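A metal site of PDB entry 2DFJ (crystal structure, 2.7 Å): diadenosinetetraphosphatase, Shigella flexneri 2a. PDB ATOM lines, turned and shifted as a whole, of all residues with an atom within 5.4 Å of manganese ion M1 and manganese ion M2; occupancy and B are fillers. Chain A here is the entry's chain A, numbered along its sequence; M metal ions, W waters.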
ATOM      1  N   ASP A   8      25.655  15.053 -23.820  1.00  0.00           N
ATOM      2  CA  ASP A   8      25.981  13.926 -24.714  1.00  0.00           C
ATOM      3  C   ASP A   8      27.285  14.035 -25.469  1.00  0.00           C
ATOM      4  O   ASP A   8      27.463  14.932 -26.302  1.00  0.00           O
ATOM      5  CB  ASP A   8      24.837  13.680 -25.692  1.00  0.00           C
ATOM      6  CG  ASP A   8      23.630  13.089 -25.022  1.00  0.00           C
ATOM      7  OD1 ASP A   8      23.549  13.223 -23.792  1.00  0.00           O
ATOM      8  OD2 ASP A   8      22.782  12.485 -25.693  1.00  0.00           O
ATOM      9  N   HIS A  10      28.832  12.181 -27.954  1.00  0.00           N
ATOM     10  CA  HIS A  10      28.692  11.050 -28.856  1.00  0.00           C
ATOM     11  C   HIS A  10      29.989  10.700 -29.543  1.00  0.00           C
ATOM     12  O   HIS A  10      30.276  11.200 -30.627  1.00  0.00           O
ATOM     13  CB  HIS A  10      27.621  11.333 -29.872  1.00  0.00           C
ATOM     14  CG  HIS A  10      26.239  11.124 -29.322  1.00  0.00           C
ATOM     15  ND1 HIS A  10      25.768   9.844 -28.987  1.00  0.00           N
ATOM     16  CD2 HIS A  10      25.235  11.995 -29.026  1.00  0.00           C
ATOM     17  CE1 HIS A  10      24.565   9.901 -28.570  1.00  0.00           C
ATOM     18  NE2 HIS A  10      24.170  11.238 -28.535  1.00  0.00           N
ATOM     19  N   ASP A  37      25.245   8.618 -23.093  1.00  0.00           N
ATOM     20  CA  ASP A  37      25.463   8.593 -24.545  1.00  0.00           C
ATOM     21  C   ASP A  37      26.886   9.037 -24.858  1.00  0.00           C
ATOM     22  O   ASP A  37      27.125   9.998 -25.589  1.00  0.00           O
ATOM     23  CB  ASP A  37      24.415   9.413 -25.304  1.00  0.00           C
ATOM     24  CG  ASP A  37      23.113   8.663 -25.505  1.00  0.00           C
ATOM     25  OD1 ASP A  37      23.006   7.484 -25.083  1.00  0.00           O
ATOM     26  OD2 ASP A  37      22.167   9.253 -26.077  1.00  0.00           O
ATOM     27  N   ARG A  41      27.406   8.495 -32.389  1.00  0.00           N
ATOM     28  CA  ARG A  41      27.690   8.594 -33.834  1.00  0.00           C
ATOM     29  C   ARG A  41      29.106   8.976 -34.193  1.00  0.00           C
ATOM     30  O   ARG A  41      29.617   8.537 -35.215  1.00  0.00           O
ATOM     31  CB  ARG A  41      26.743   9.563 -34.559  1.00  0.00           C
ATOM     32  CG  ARG A  41      25.274   9.558 -34.116  1.00  0.00           C
ATOM     33  CD  ARG A  41      24.557   8.207 -34.366  1.00  0.00           C
ATOM     34  NE  ARG A  41      23.132   8.207 -33.990  1.00  0.00           N
ATOM     35  CZ  ARG A  41      22.555   8.910 -32.995  1.00  0.00           C
ATOM     36  NH1 ARG A  41      23.275   9.714 -32.185  1.00  0.00           N
ATOM     37  NH2 ARG A  41      21.239   8.793 -32.794  1.00  0.00           N
ATOM     38  N   GLY A  64      22.954   6.396 -20.945  1.00  0.00           N
ATOM     39  CA  GLY A  64      21.906   6.769 -21.908  1.00  0.00           C
ATOM     40  C   GLY A  64      21.422   5.620 -22.786  1.00  0.00           C
ATOM     41  O   GLY A  64      21.927   4.487 -22.695  1.00  0.00           O
ATOM     42  N   ASN A  65      20.436   5.907 -23.649  1.00  0.00           N
ATOM     43  CA  ASN A  65      19.897   4.906 -24.581  1.00  0.00           C
ATOM     44  C   ASN A  65      20.948   4.263 -25.476  1.00  0.00           C
ATOM     45  O   ASN A  65      20.934   3.049 -25.685  1.00  0.00           O
ATOM     46  CB  ASN A  65      18.749   5.502 -25.418  1.00  0.00           C
ATOM     47  CG  ASN A  65      19.109   6.875 -26.018  1.00  0.00           C
ATOM     48  OD1 ASN A  65      19.552   7.771 -25.303  1.00  0.00           O
ATOM     49  ND2 ASN A  65      18.882   7.037 -27.321  1.00  0.00           N
ATOM     50  N   HIS A  66      21.869   5.068 -26.005  1.00  0.00           N
ATOM     51  CA  HIS A  66      22.943   4.532 -26.847  1.00  0.00           C
ATOM     52  C   HIS A  66      23.981   3.696 -26.099  1.00  0.00           C
ATOM     53  O   HIS A  66      24.552   2.773 -26.675  1.00  0.00           O
ATOM     54  CB  HIS A  66      23.651   5.632 -27.619  1.00  0.00           C
ATOM     55  CG  HIS A  66      22.828   6.177 -28.746  1.00  0.00           C
ATOM     56  ND1 HIS A  66      21.884   7.164 -28.564  1.00  0.00           N
ATOM     57  CD2 HIS A  66      22.809   5.860 -30.062  1.00  0.00           C
ATOM     58  CE1 HIS A  66      21.324   7.443 -29.728  1.00  0.00           C
ATOM     59  NE2 HIS A  66      21.870   6.675 -30.652  1.00  0.00           N
ATOM     60  N   HIS A 120      19.734  10.548 -17.511  1.00  0.00           N
ATOM     61  CA  HIS A 120      19.987  10.809 -18.927  1.00  0.00           C
ATOM     62  C   HIS A 120      18.919  11.663 -19.617  1.00  0.00           C
ATOM     63  O   HIS A 120      19.254  12.657 -20.250  1.00  0.00           O
ATOM     64  CB  HIS A 120      20.209   9.517 -19.700  1.00  0.00           C
ATOM     65  CG  HIS A 120      20.449   9.728 -21.165  1.00  0.00           C
ATOM     66  ND1 HIS A 120      21.540  10.408 -21.656  1.00  0.00           N
ATOM     67  CD2 HIS A 120      19.738   9.330 -22.251  1.00  0.00           C
ATOM     68  CE1 HIS A 120      21.506  10.415 -22.973  1.00  0.00           C
ATOM     69  NE2 HIS A 120      20.422   9.763 -23.356  1.00  0.00           N
ATOM     70  N   THR A 181      15.858   7.017 -19.959  1.00  0.00           N
ATOM     71  CA  THR A 181      16.718   7.074 -21.146  1.00  0.00           C
ATOM     72  C   THR A 181      16.055   7.391 -22.491  1.00  0.00           C
ATOM     73  O   THR A 181      16.762   7.532 -23.496  1.00  0.00           O
ATOM     74  CB  THR A 181      17.571   5.785 -21.316  1.00  0.00           C
ATOM     75  OG1 THR A 181      16.755   4.705 -21.773  1.00  0.00           O
ATOM     76  CG2 THR A 181      18.228   5.382 -20.010  1.00  0.00           C
ATOM     77  N   GLY A 226      20.369  15.295 -20.506  1.00  0.00           N
ATOM     78  CA  GLY A 226      20.730  15.637 -21.880  1.00  0.00           C
ATOM     79  C   GLY A 226      20.504  14.535 -22.883  1.00  0.00           C
ATOM     80  O   GLY A 226      21.432  13.844 -23.269  1.00  0.00           O
ATOM     81  N   HIS A 227      19.283  14.349 -23.328  1.00  0.00           N
ATOM     82  CA  HIS A 227      19.015  13.318 -24.307  1.00  0.00           C
ATOM     83  C   HIS A 227      18.336  14.048 -25.446  1.00  0.00           C
ATOM     84  O   HIS A 227      18.715  13.937 -26.610  1.00  0.00           O
ATOM     85  CB  HIS A 227      18.145  12.241 -23.653  1.00  0.00           C
ATOM     86  CG  HIS A 227      17.334  11.423 -24.612  1.00  0.00           C
ATOM     87  ND1 HIS A 227      17.903  10.627 -25.588  1.00  0.00           N
ATOM     88  CD2 HIS A 227      15.984  11.228 -24.682  1.00  0.00           C
ATOM     89  CE1 HIS A 227      16.940  10.006 -26.251  1.00  0.00           C
ATOM     90  NE2 HIS A 227      15.760  10.347 -25.720  1.00  0.00           N
ATOM     91  N   ASP A 244      22.392  18.728 -23.508  1.00  0.00           N
ATOM     92  CA  ASP A 244      22.596  18.134 -24.837  1.00  0.00           C
ATOM     93  C   ASP A 244      22.372  19.135 -25.976  1.00  0.00           C
ATOM     94  O   ASP A 244      21.232  19.542 -26.270  1.00  0.00           O
ATOM     95  CB  ASP A 244      21.721  16.906 -25.040  1.00  0.00           C
ATOM     96  CG  ASP A 244      22.120  16.096 -26.264  1.00  0.00           C
ATOM     97  OD1 ASP A 244      22.849  16.614 -27.147  1.00  0.00           O
ATOM     98  OD2 ASP A 244      21.686  14.929 -26.347  1.00  0.00           O
HETATM   99 MN    MN M   1      22.352  11.234 -27.439  1.00  0.00          MN
HETATM  100 MN    MN M   2      19.918   9.828 -25.515  1.00  0.00          MN
HETATM  101  O   HOH W   1      19.634   9.688 -27.782  1.00  0.00           O
HETATM  102  O   HOH W   2      21.359  10.211 -29.520  1.00  0.00           O
HETATM  103  O   HOH W   3      20.628  11.801 -26.724  1.00  0.00           O
HETATM  104  O   HOH W   4      22.487  13.255 -28.468  1.00  0.00           O
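Manganese ion M2 is bound by OD1 of Asn 65 (2.1 Å), ND1 of His 227 (2.2 Å), NE2 of His 120 (2.2 Å), water W1 (2.3 Å), OD2 of Asp 37 (2.4 Å) and water W3 (2.4 Å).
Manganese ion M1 is bound by water W3 (2.0 Å), a ring nitrogen (NE2) of His 10 (2.1 Å), the side-chain carboxylate of Asp 8 (2.2 Å), water W4 (2.3 Å), the side-chain carboxylate of Asp 37 (2.4 Å) and water W2 (2.5 Å). Manganese ion M1 has six donor atoms within binding distance.
Within 4 Å of manganese ion M2: Asp 8, Asp 37, Asn 65, His 120 and His 227. The nearest printed residue that does not touch manganese ion M2 is Thr 181 (4.4 Å).
The backbone carbonyl oxygen of His 120 is in hydrogen-bond range of the backbone NH of Gly 226 (2.9 Å). O of Thr 181 sits close to OD1 of Asn 65, at 3.3 Å. OD1 of Asp 37 sits at hydrogen-bond distance from N of His 66 (2.8 Å). ND1 of His 66 sits at hydrogen-bond distance from ND2 of Asn 65.
Water W3 bridges the backbone carbonyl oxygen of His 227 (2.9 Å) and the side-chain carboxylate of Asp 244 (3.3 Å). Water W2 lies within hydrogen-bond range of a ring nitrogen (ND1) of His 66 (3.2 Å) and the guanidinium group (NH1) of Arg 41 (3.3 Å). Water W1 lies within hydrogen-bond range of the side-chain amide nitrogen of Asn 65 (2.8 Å) and a ring nitrogen (ND1) of His 66 (3.5 Å).
Residues that only touch manganese ion M1: Asp 244. Four residues have an atom within 4 Å of manganese ion M1: Asp 8, His 10, Asp 37 and Asp 244.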
